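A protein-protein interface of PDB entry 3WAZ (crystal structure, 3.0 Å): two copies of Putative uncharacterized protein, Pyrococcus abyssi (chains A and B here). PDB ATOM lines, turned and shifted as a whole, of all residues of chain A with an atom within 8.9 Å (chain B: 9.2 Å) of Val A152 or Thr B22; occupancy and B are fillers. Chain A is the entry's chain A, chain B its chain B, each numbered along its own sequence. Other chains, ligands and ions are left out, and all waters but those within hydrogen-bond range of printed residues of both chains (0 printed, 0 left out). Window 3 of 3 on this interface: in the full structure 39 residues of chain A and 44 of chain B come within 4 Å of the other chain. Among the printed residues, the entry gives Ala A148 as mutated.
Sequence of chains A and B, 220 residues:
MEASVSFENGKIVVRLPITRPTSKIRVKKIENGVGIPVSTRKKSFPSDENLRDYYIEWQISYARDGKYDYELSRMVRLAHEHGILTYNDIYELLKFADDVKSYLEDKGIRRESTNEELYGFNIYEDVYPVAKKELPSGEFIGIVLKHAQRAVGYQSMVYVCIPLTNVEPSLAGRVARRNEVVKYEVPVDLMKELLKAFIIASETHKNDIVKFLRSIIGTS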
ATOM      1  N   LYS A 146      17.540 -17.201 -10.455  1.00  0.00           N
ATOM      2  CA  LYS A 146      16.956 -18.173 -11.371  1.00  0.00           C
ATOM      3  C   LYS A 146      15.444 -18.003 -11.436  1.00  0.00           C
ATOM      4  O   LYS A 146      14.860 -17.243 -10.662  1.00  0.00           O
ATOM      5  CB  LYS A 146      17.308 -19.600 -10.952  1.00  0.00           C
ATOM      6  CG  LYS A 146      16.627 -20.058  -9.678  1.00  0.00           C
ATOM      7  CD  LYS A 146      16.849 -21.544  -9.422  1.00  0.00           C
ATOM      8  CE  LYS A 146      18.318 -21.863  -9.204  1.00  0.00           C
ATOM      9  NZ  LYS A 146      18.531 -23.308  -8.917  1.00  0.00           N
ATOM     10  N   HIS A 147      14.814 -18.719 -12.360  1.00  0.00           N
ATOM     11  CA  HIS A 147      13.379 -18.602 -12.572  1.00  0.00           C
ATOM     12  C   HIS A 147      12.591 -19.157 -11.391  1.00  0.00           C
ATOM     13  O   HIS A 147      12.983 -20.156 -10.786  1.00  0.00           O
ATOM     14  CB  HIS A 147      12.978 -19.326 -13.855  1.00  0.00           C
ATOM     15  CG  HIS A 147      11.638 -18.921 -14.382  1.00  0.00           C
ATOM     16  ND1 HIS A 147      10.455 -19.321 -13.799  1.00  0.00           N
ATOM     17  CD2 HIS A 147      11.294 -18.150 -15.441  1.00  0.00           C
ATOM     18  CE1 HIS A 147       9.440 -18.813 -14.475  1.00  0.00           C
ATOM     19  NE2 HIS A 147       9.921 -18.099 -15.476  1.00  0.00           N
ATOM     20  N   ALA A 148      11.483 -18.499 -11.068  1.00  0.00           N
ATOM     21  CA  ALA A 148      10.596 -18.970 -10.013  1.00  0.00           C
ATOM     22  C   ALA A 148      10.035 -20.332 -10.385  1.00  0.00           C
ATOM     23  O   ALA A 148       9.789 -20.611 -11.558  1.00  0.00           O
ATOM     24  CB  ALA A 148       9.471 -17.981  -9.787  1.00  0.00           C
ATOM     25  N   GLN A 149       9.839 -21.180  -9.381  1.00  0.00           N
ATOM     26  CA  GLN A 149       9.346 -22.532  -9.607  1.00  0.00           C
ATOM     27  C   GLN A 149       7.956 -22.536 -10.229  1.00  0.00           C
ATOM     28  O   GLN A 149       7.695 -23.272 -11.180  1.00  0.00           O
ATOM     29  CB  GLN A 149       9.322 -23.318  -8.296  1.00  0.00           C
ATOM     30  CG  GLN A 149       8.769 -24.724  -8.441  1.00  0.00           C
ATOM     31  CD  GLN A 149       8.534 -25.401  -7.108  1.00  0.00           C
ATOM     32  OE1 GLN A 149       8.764 -24.814  -6.051  1.00  0.00           O
ATOM     33  NE2 GLN A 149       8.070 -26.643  -7.150  1.00  0.00           N
ATOM     34  N   ARG A 150       7.067 -21.707  -9.692  1.00  0.00           N
ATOM     35  CA  ARG A 150       5.680 -21.687 -10.139  1.00  0.00           C
ATOM     36  C   ARG A 150       5.268 -20.354 -10.764  1.00  0.00           C
ATOM     37  O   ARG A 150       4.441 -20.320 -11.677  1.00  0.00           O
ATOM     38  CB  ARG A 150       4.742 -22.046  -8.984  1.00  0.00           C
ATOM     39  CG  ARG A 150       4.928 -23.462  -8.458  1.00  0.00           C
ATOM     40  CD  ARG A 150       3.815 -23.861  -7.500  1.00  0.00           C
ATOM     41  NE  ARG A 150       4.049 -23.392  -6.136  1.00  0.00           N
ATOM     42  CZ  ARG A 150       4.555 -24.146  -5.165  1.00  0.00           C
ATOM     43  NH1 ARG A 150       4.882 -25.409  -5.408  1.00  0.00           N
ATOM     44  NH2 ARG A 150       4.731 -23.641  -3.950  1.00  0.00           N
ATOM     45  N   ALA A 151       5.849 -19.262 -10.278  1.00  0.00           N
ATOM     46  CA  ALA A 151       5.470 -17.930 -10.743  1.00  0.00           C
ATOM     47  C   ALA A 151       6.135 -17.551 -12.064  1.00  0.00           C
ATOM     48  O   ALA A 151       6.708 -18.396 -12.755  1.00  0.00           O
ATOM     49  CB  ALA A 151       5.774 -16.891  -9.678  1.00  0.00           C
ATOM     50  N   VAL A 152       6.048 -16.270 -12.407  1.00  0.00           N
ATOM     51  CA  VAL A 152       6.620 -15.755 -13.644  1.00  0.00           C
ATOM     52  C   VAL A 152       7.807 -14.847 -13.359  1.00  0.00           C
ATOM     53  O   VAL A 152       7.694 -13.887 -12.597  1.00  0.00           O
ATOM     54  CB  VAL A 152       5.583 -14.953 -14.448  1.00  0.00           C
ATOM     55  CG1 VAL A 152       6.213 -14.384 -15.706  1.00  0.00           C
ATOM     56  CG2 VAL A 152       4.390 -15.820 -14.795  1.00  0.00           C
ATOM     57  N   GLY A 153       8.946 -15.151 -13.971  1.00  0.00           N
ATOM     58  CA  GLY A 153      10.115 -14.301 -13.849  1.00  0.00           C
ATOM     59  C   GLY A 153      11.221 -14.882 -12.993  1.00  0.00           C
ATOM     60  O   GLY A 153      11.130 -16.013 -12.516  1.00  0.00           O
ATOM     61  N   TYR A 154      12.271 -14.093 -12.794  1.00  0.00           N
ATOM     62  CA  TYR A 154      13.446 -14.549 -12.064  1.00  0.00           C
ATOM     63  C   TYR A 154      13.565 -13.883 -10.698  1.00  0.00           C
ATOM     64  O   TYR A 154      13.332 -12.683 -10.558  1.00  0.00           O
ATOM     65  CB  TYR A 154      14.708 -14.290 -12.885  1.00  0.00           C
ATOM     66  CG  TYR A 154      14.670 -14.915 -14.260  1.00  0.00           C
ATOM     67  CD1 TYR A 154      14.210 -14.200 -15.359  1.00  0.00           C
ATOM     68  CD2 TYR A 154      15.094 -16.220 -14.459  1.00  0.00           C
ATOM     69  CE1 TYR A 154      14.174 -14.770 -16.616  1.00  0.00           C
ATOM     70  CE2 TYR A 154      15.061 -16.799 -15.711  1.00  0.00           C
ATOM     71  CZ  TYR A 154      14.600 -16.071 -16.785  1.00  0.00           C
ATOM     72  OH  TYR A 154      14.567 -16.644 -18.035  1.00  0.00           O
ATOM     73  N   GLN A 155      13.933 -14.675  -9.697  1.00  0.00           N
ATOM     74  CA  GLN A 155      14.098 -14.175  -8.339  1.00  0.00           C
ATOM     75  C   GLN A 155      15.462 -14.559  -7.784  1.00  0.00           C
ATOM     76  O   GLN A 155      16.138 -15.439  -8.319  1.00  0.00           O
ATOM     77  CB  GLN A 155      13.016 -14.743  -7.421  1.00  0.00           C
ATOM     78  CG  GLN A 155      11.595 -14.531  -7.900  1.00  0.00           C
ATOM     79  CD  GLN A 155      10.574 -15.082  -6.927  1.00  0.00           C
ATOM     80  OE1 GLN A 155      10.922 -15.547  -5.839  1.00  0.00           O
ATOM     81  NE2 GLN A 155       9.305 -15.034  -7.311  1.00  0.00           N
ATOM     82  N   PRO B  17      -2.040 -20.122 -28.261  1.00  0.00           N
ATOM     83  CA  PRO B  17      -2.536 -19.239 -27.201  1.00  0.00           C
ATOM     84  C   PRO B  17      -1.392 -18.426 -26.605  1.00  0.00           C
ATOM     85  O   PRO B  17      -0.339 -18.982 -26.295  1.00  0.00           O
ATOM     86  CB  PRO B  17      -3.091 -20.218 -26.164  1.00  0.00           C
ATOM     87  CG  PRO B  17      -2.317 -21.470 -26.378  1.00  0.00           C
ATOM     88  CD  PRO B  17      -2.051 -21.538 -27.853  1.00  0.00           C
ATOM     89  N   ILE B  18      -1.597 -17.123 -26.449  1.00  0.00           N
ATOM     90  CA  ILE B  18      -0.531 -16.233 -26.003  1.00  0.00           C
ATOM     91  C   ILE B  18      -0.887 -15.489 -24.719  1.00  0.00           C
ATOM     92  O   ILE B  18      -0.326 -14.431 -24.431  1.00  0.00           O
ATOM     93  CB  ILE B  18      -0.180 -15.208 -27.092  1.00  0.00           C
ATOM     94  CG1 ILE B  18      -1.423 -14.406 -27.476  1.00  0.00           C
ATOM     95  CG2 ILE B  18       0.398 -15.907 -28.312  1.00  0.00           C
ATOM     96  CD1 ILE B  18      -1.191 -13.432 -28.596  1.00  0.00           C
ATOM     97  N   THR B  19      -1.819 -16.043 -23.951  1.00  0.00           N
ATOM     98  CA  THR B  19      -2.214 -15.441 -22.683  1.00  0.00           C
ATOM     99  C   THR B  19      -2.002 -16.409 -21.525  1.00  0.00           C
ATOM    100  O   THR B  19      -2.603 -16.265 -20.463  1.00  0.00           O
ATOM    101  CB  THR B  19      -3.681 -14.969 -22.704  1.00  0.00           C
ATOM    102  OG1 THR B  19      -4.535 -16.062 -23.065  1.00  0.00           O
ATOM    103  CG2 THR B  19      -3.861 -13.842 -23.709  1.00  0.00           C
ATOM    104  N   ARG B  20      -1.142 -17.398 -21.741  1.00  0.00           N
ATOM    105  CA  ARG B  20      -0.774 -18.335 -20.689  1.00  0.00           C
ATOM    106  C   ARG B  20       0.737 -18.317 -20.498  1.00  0.00           C
ATOM    107  O   ARG B  20       1.450 -19.147 -21.062  1.00  0.00           O
ATOM    108  CB  ARG B  20      -1.251 -19.747 -21.030  1.00  0.00           C
ATOM    109  CG  ARG B  20      -2.759 -19.879 -21.186  1.00  0.00           C
ATOM    110  CD  ARG B  20      -3.490 -19.457 -19.921  1.00  0.00           C
ATOM    111  NE  ARG B  20      -4.897 -19.844 -19.947  1.00  0.00           N
ATOM    112  CZ  ARG B  20      -5.873 -19.090 -20.444  1.00  0.00           C
ATOM    113  NH1 ARG B  20      -7.125 -19.526 -20.425  1.00  0.00           N
ATOM    114  NH2 ARG B  20      -5.598 -17.901 -20.962  1.00  0.00           N
ATOM    115  N   PRO B  21       1.231 -17.362 -19.694  1.00  0.00           N
ATOM    116  CA  PRO B  21       2.667 -17.126 -19.507  1.00  0.00           C
ATOM    117  C   PRO B  21       3.343 -18.196 -18.657  1.00  0.00           C
ATOM    118  O   PRO B  21       4.557 -18.138 -18.461  1.00  0.00           O
ATOM    119  CB  PRO B  21       2.700 -15.787 -18.773  1.00  0.00           C
ATOM    120  CG  PRO B  21       1.429 -15.765 -18.006  1.00  0.00           C
ATOM    121  CD  PRO B  21       0.416 -16.438 -18.887  1.00  0.00           C
ATOM    122  N   THR B  22       2.568 -19.149 -18.152  1.00  0.00           N
ATOM    123  CA  THR B  22       3.121 -20.233 -17.349  1.00  0.00           C
ATOM    124  C   THR B  22       2.936 -21.583 -18.031  1.00  0.00           C
ATOM    125  O   THR B  22       3.195 -22.629 -17.437  1.00  0.00           O
ATOM    126  CB  THR B  22       2.492 -20.281 -15.948  1.00  0.00           C
ATOM    127  OG1 THR B  22       1.070 -20.151 -16.058  1.00  0.00           O
ATOM    128  CG2 THR B  22       3.029 -19.151 -15.089  1.00  0.00           C
ATOM    129  N   SER B  23       2.482 -21.550 -19.280  1.00  0.00           N
ATOM    130  CA  SER B  23       2.325 -22.763 -20.072  1.00  0.00           C
ATOM    131  C   SER B  23       3.630 -23.089 -20.785  1.00  0.00           C
ATOM    132  O   SER B  23       4.682 -22.547 -20.447  1.00  0.00           O
ATOM    133  CB  SER B  23       1.201 -22.591 -21.094  1.00  0.00           C
ATOM    134  OG  SER B  23       1.499 -21.553 -22.012  1.00  0.00           O
ATOM    135  N   LYS B  24       3.563 -23.978 -21.770  1.00  0.00           N
ATOM    136  CA  LYS B  24       4.733 -24.286 -22.582  1.00  0.00           C
ATOM    137  C   LYS B  24       4.838 -23.310 -23.745  1.00  0.00           C
ATOM    138  O   LYS B  24       5.786 -23.358 -24.528  1.00  0.00           O
ATOM    139  CB  LYS B  24       4.700 -25.733 -23.078  1.00  0.00           C
ATOM    140  CG  LYS B  24       3.457 -26.109 -23.865  1.00  0.00           C
ATOM    141  CD  LYS B  24       3.458 -27.595 -24.191  1.00  0.00           C
ATOM    142  CE  LYS B  24       2.165 -28.024 -24.863  1.00  0.00           C
ATOM    143  NZ  LYS B  24       2.130 -29.496 -25.092  1.00  0.00           N
ATOM    144  N   ILE B  25       3.854 -22.421 -23.846  1.00  0.00           N
ATOM    145  CA  ILE B  25       3.867 -21.359 -24.842  1.00  0.00           C
ATOM    146  C   ILE B  25       3.867 -20.003 -24.148  1.00  0.00           C
ATOM    147  O   ILE B  25       2.846 -19.565 -23.622  1.00  0.00           O
ATOM    148  CB  ILE B  25       2.656 -21.452 -25.784  1.00  0.00           C
ATOM    149  CG1 ILE B  25       2.647 -22.802 -26.503  1.00  0.00           C
ATOM    150  CG2 ILE B  25       2.673 -20.312 -26.790  1.00  0.00           C
ATOM    151  CD1 ILE B  25       1.420 -23.030 -27.355  1.00  0.00           C
ATOM    152  N   ARG B  26       5.023 -19.347 -24.142  1.00  0.00           N
ATOM    153  CA  ARG B  26       5.179 -18.083 -23.434  1.00  0.00           C
ATOM    154  C   ARG B  26       5.680 -16.978 -24.357  1.00  0.00           C
ATOM    155  O   ARG B  26       6.487 -17.223 -25.254  1.00  0.00           O
ATOM    156  CB  ARG B  26       6.143 -18.254 -22.258  1.00  0.00           C
ATOM    157  CG  ARG B  26       5.826 -19.449 -21.372  1.00  0.00           C
ATOM    158  CD  ARG B  26       6.845 -19.607 -20.254  1.00  0.00           C
ATOM    159  NE  ARG B  26       6.568 -20.781 -19.432  1.00  0.00           N
ATOM    160  CZ  ARG B  26       7.223 -21.085 -18.318  1.00  0.00           C
ATOM    161  NH1 ARG B  26       8.199 -20.297 -17.887  1.00  0.00           N
ATOM    162  NH2 ARG B  26       6.902 -22.175 -17.633  1.00  0.00           N
ATOM    163  N   VAL B  27       5.194 -15.761 -24.133  1.00  0.00           N
ATOM    164  CA  VAL B  27       5.646 -14.606 -24.898  1.00  0.00           C
ATOM    165  C   VAL B  27       6.785 -13.908 -24.168  1.00  0.00           C
ATOM    166  O   VAL B  27       6.615 -13.427 -23.047  1.00  0.00           O
ATOM    167  CB  VAL B  27       4.508 -13.598 -25.133  1.00  0.00           C
ATOM    168  CG1 VAL B  27       5.045 -12.338 -25.795  1.00  0.00           C
ATOM    169  CG2 VAL B  27       3.411 -14.225 -25.976  1.00  0.00           C
ATOM    170  N   LYS B  28       7.947 -13.856 -24.809  1.00  0.00           N
ATOM    171  CA  LYS B  28       9.117 -13.235 -24.204  1.00  0.00           C
ATOM    172  C   LYS B  28       9.731 -12.167 -25.102  1.00  0.00           C
ATOM    173  O   LYS B  28       9.681 -12.265 -26.328  1.00  0.00           O
ATOM    174  CB  LYS B  28      10.165 -14.292 -23.849  1.00  0.00           C
ATOM    175  CG  LYS B  28       9.734 -15.237 -22.741  1.00  0.00           C
ATOM    176  CD  LYS B  28      10.865 -16.161 -22.330  1.00  0.00           C
ATOM    177  CE  LYS B  28      10.482 -16.993 -21.119  1.00  0.00           C
ATOM    178  NZ  LYS B  28      11.586 -17.901 -20.703  1.00  0.00           N
ATOM    179  N   ILE B  36      12.860 -12.256 -21.866  1.00  0.00           N
ATOM    180  CA  ILE B  36      12.223 -11.688 -20.684  1.00  0.00           C
ATOM    181  C   ILE B  36      10.704 -11.793 -20.809  1.00  0.00           C
ATOM    182  O   ILE B  36      10.136 -11.415 -21.833  1.00  0.00           O
ATOM    183  CB  ILE B  36      12.646 -10.213 -20.466  1.00  0.00           C
ATOM    184  CG1 ILE B  36      13.909 -10.137 -19.603  1.00  0.00           C
ATOM    185  CG2 ILE B  36      11.536  -9.412 -19.801  1.00  0.00           C
ATOM    186  CD1 ILE B  36      15.172 -10.590 -20.302  1.00  0.00           C
ATOM    187  N   PRO B  37      10.042 -12.315 -19.762  1.00  0.00           N
ATOM    188  CA  PRO B  37       8.593 -12.543 -19.752  1.00  0.00           C
ATOM    189  C   PRO B  37       7.786 -11.273 -20.011  1.00  0.00           C
ATOM    190  O   PRO B  37       8.218 -10.177 -19.650  1.00  0.00           O
ATOM    191  CB  PRO B  37       8.328 -13.061 -18.332  1.00  0.00           C
ATOM    192  CG  PRO B  37       9.506 -12.618 -17.530  1.00  0.00           C
ATOM    193  CD  PRO B  37      10.661 -12.671 -18.475  1.00  0.00           C
ATOM    194  N   VAL B  38       6.624 -11.432 -20.637  1.00  0.00           N
ATOM    195  CA  VAL B  38       5.784 -10.298 -21.007  1.00  0.00           C
ATOM    196  C   VAL B  38       4.326 -10.520 -20.614  1.00  0.00           C
ATOM    197  O   VAL B  38       3.732 -11.546 -20.949  1.00  0.00           O
ATOM    198  CB  VAL B  38       5.854 -10.022 -22.527  1.00  0.00           C
ATOM    199  CG1 VAL B  38       4.795  -9.010 -22.940  1.00  0.00           C
ATOM    200  CG2 VAL B  38       7.238  -9.535 -22.918  1.00  0.00           C
ATOM    201  N   SER B  39       3.759  -9.555 -19.898  1.00  0.00           N
ATOM    202  CA  SER B  39       2.336  -9.569 -19.585  1.00  0.00           C
ATOM    203  C   SER B  39       1.551  -9.031 -20.777  1.00  0.00           C
ATOM    204  O   SER B  39       1.324  -7.827 -20.893  1.00  0.00           O
ATOM    205  CB  SER B  39       2.050  -8.732 -18.337  1.00  0.00           C
ATOM    206  OG  SER B  39       2.702  -9.271 -17.200  1.00  0.00           O
ATOM    207  N   THR B  40       1.140  -9.937 -21.659  1.00  0.00           N
ATOM    208  CA  THR B  40       0.492  -9.567 -22.915  1.00  0.00           C
ATOM    209  C   THR B  40      -0.845  -8.852 -22.724  1.00  0.00           C
ATOM    210  O   THR B  40      -1.295  -8.120 -23.607  1.00  0.00           O
ATOM    211  CB  THR B  40       0.280 -10.801 -23.815  1.00  0.00           C
ATOM    212  OG1 THR B  40      -0.527 -11.766 -23.127  1.00  0.00           O
ATOM    213  CG2 THR B  40       1.615 -11.432 -24.176  1.00  0.00           C
ATOM    214  N   GLU B  57       7.885 -18.184 -27.166  1.00  0.00           N
ATOM    215  CA  GLU B  57       8.692 -19.311 -26.717  1.00  0.00           C
ATOM    216  C   GLU B  57       7.814 -20.540 -26.506  1.00  0.00           C
ATOM    217  O   GLU B  57       6.972 -20.569 -25.611  1.00  0.00           O
ATOM    218  CB  GLU B  57       9.439 -18.966 -25.429  1.00  0.00           C
ATOM    219  CG  GLU B  57      10.444 -20.020 -25.004  1.00  0.00           C
ATOM    220  CD  GLU B  57      11.059 -19.724 -23.653  1.00  0.00           C
ATOM    221  OE1 GLU B  57      10.343 -19.841 -22.635  1.00  0.00           O
ATOM    222  OE2 GLU B  57      12.256 -19.370 -23.607  1.00  0.00           O
ATOM    223  N   GLN B  59       7.899 -24.551 -25.881  1.00  0.00           N
ATOM    224  CA  GLN B  59       8.555 -25.818 -25.578  1.00  0.00           C
ATOM    225  C   GLN B  59       7.738 -26.949 -26.186  1.00  0.00           C
ATOM    226  O   GLN B  59       6.984 -27.636 -25.496  1.00  0.00           O
ATOM    227  CB  GLN B  59       8.725 -26.014 -24.071  1.00  0.00           C
ATOM    228  CG  GLN B  59       9.646 -27.171 -23.716  1.00  0.00           C
ATOM    229  CD  GLN B  59      10.013 -27.201 -22.248  1.00  0.00           C
ATOM    230  OE1 GLN B  59       9.521 -26.398 -21.456  1.00  0.00           O
ATOM    231  NE2 GLN B  59      10.886 -28.129 -21.877  1.00  0.00           N
ATOM    232  N   GLN B 149      11.534 -29.354 -14.590  1.00  0.00           N
ATOM    233  CA  GLN B 149      10.532 -28.613 -13.833  1.00  0.00           C
ATOM    234  C   GLN B 149      10.092 -29.356 -12.577  1.00  0.00           C
ATOM    235  O   GLN B 149      10.039 -28.776 -11.494  1.00  0.00           O
ATOM    236  CB  GLN B 149       9.313 -28.313 -14.704  1.00  0.00           C
ATOM    237  CG  GLN B 149       8.186 -27.630 -13.953  1.00  0.00           C
ATOM    238  CD  GLN B 149       6.923 -27.510 -14.774  1.00  0.00           C
ATOM    239  OE1 GLN B 149       6.883 -27.915 -15.936  1.00  0.00           O
ATOM    240  NE2 GLN B 149       5.880 -26.952 -14.174  1.00  0.00           N
ATOM    241  N   ARG B 150       9.777 -30.638 -12.726  1.00  0.00           N
ATOM    242  CA  ARG B 150       9.283 -31.433 -11.606  1.00  0.00           C
ATOM    243  C   ARG B 150      10.215 -32.580 -11.220  1.00  0.00           C
ATOM    244  O   ARG B 150      10.271 -32.973 -10.054  1.00  0.00           O
ATOM    245  CB  ARG B 150       7.880 -31.966 -11.902  1.00  0.00           C
ATOM    246  CG  ARG B 150       6.804 -30.891 -11.914  1.00  0.00           C
ATOM    247  CD  ARG B 150       5.414 -31.497 -12.000  1.00  0.00           C
ATOM    248  NE  ARG B 150       5.149 -32.084 -13.310  1.00  0.00           N
ATOM    249  CZ  ARG B 150       4.513 -31.455 -14.293  1.00  0.00           C
ATOM    250  NH1 ARG B 150       4.075 -30.216 -14.113  1.00  0.00           N
ATOM    251  NH2 ARG B 150       4.313 -32.066 -15.455  1.00  0.00           N
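NE2 of His A147 sits at hydrogen-bond distance from N of Gly A153, at 3.5 Å.
NE of Arg B26 lies close to O of Pro B21, 3.5 Å away.
The backbone carbonyl oxygen (O) of Ser B23 is in hydrogen-bond range of the guanidinium group (NE) of Arg B26 (2.8 Å).
The backbone NH (N) of Glu B57 is in hydrogen-bond range of the backbone carbonyl oxygen (O) of Arg B26.
Among the printed residues, merely in contact across the chains: His A147 with Arg B26, Arg A150 with Thr B22, Val A152 with Thr B22 and Val A152 with Pro B37.
Val A152 touches just these residues of chain B: Thr B22 (3.6 Å) and Pro B37 (3.6 Å).
Thr B22 touches two residues of chain A.
No residue of chain B comes within 4 Å of Gly A153.
No residue of chain A comes within 4 Å of Pro B21.
No residue of chain A comes within 4 Å of Ser B23.
Printed residues of chain A within 4 Å of Arg B26: His A147 (3.7 Å).
Of the printed residues of chain B, Arg A150 touches Thr B22.
The nearest residue of chain A that does not touch Thr B22 is Ala A151 (4.4 Å).
Of the 21 printed residues of chain B, 3 touch a printed residue of chain A.
Printed residues of chain B that touch a printed residue of chain A: Thr B22, Arg B26 and Pro B37.
Of the 10 printed residues of chain A, 3 touch a printed residue of chain B.
Hydrophobic or aromatic side chains of chain A within 4 Å of the printed part of chain B: His A147 and Val A152.
Among the printed residues, no Asp or Glu carboxylate lies within 4 Å of a Lys or Arg side-chain nitrogen of the other chain.
2 positions are printed for both chains.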
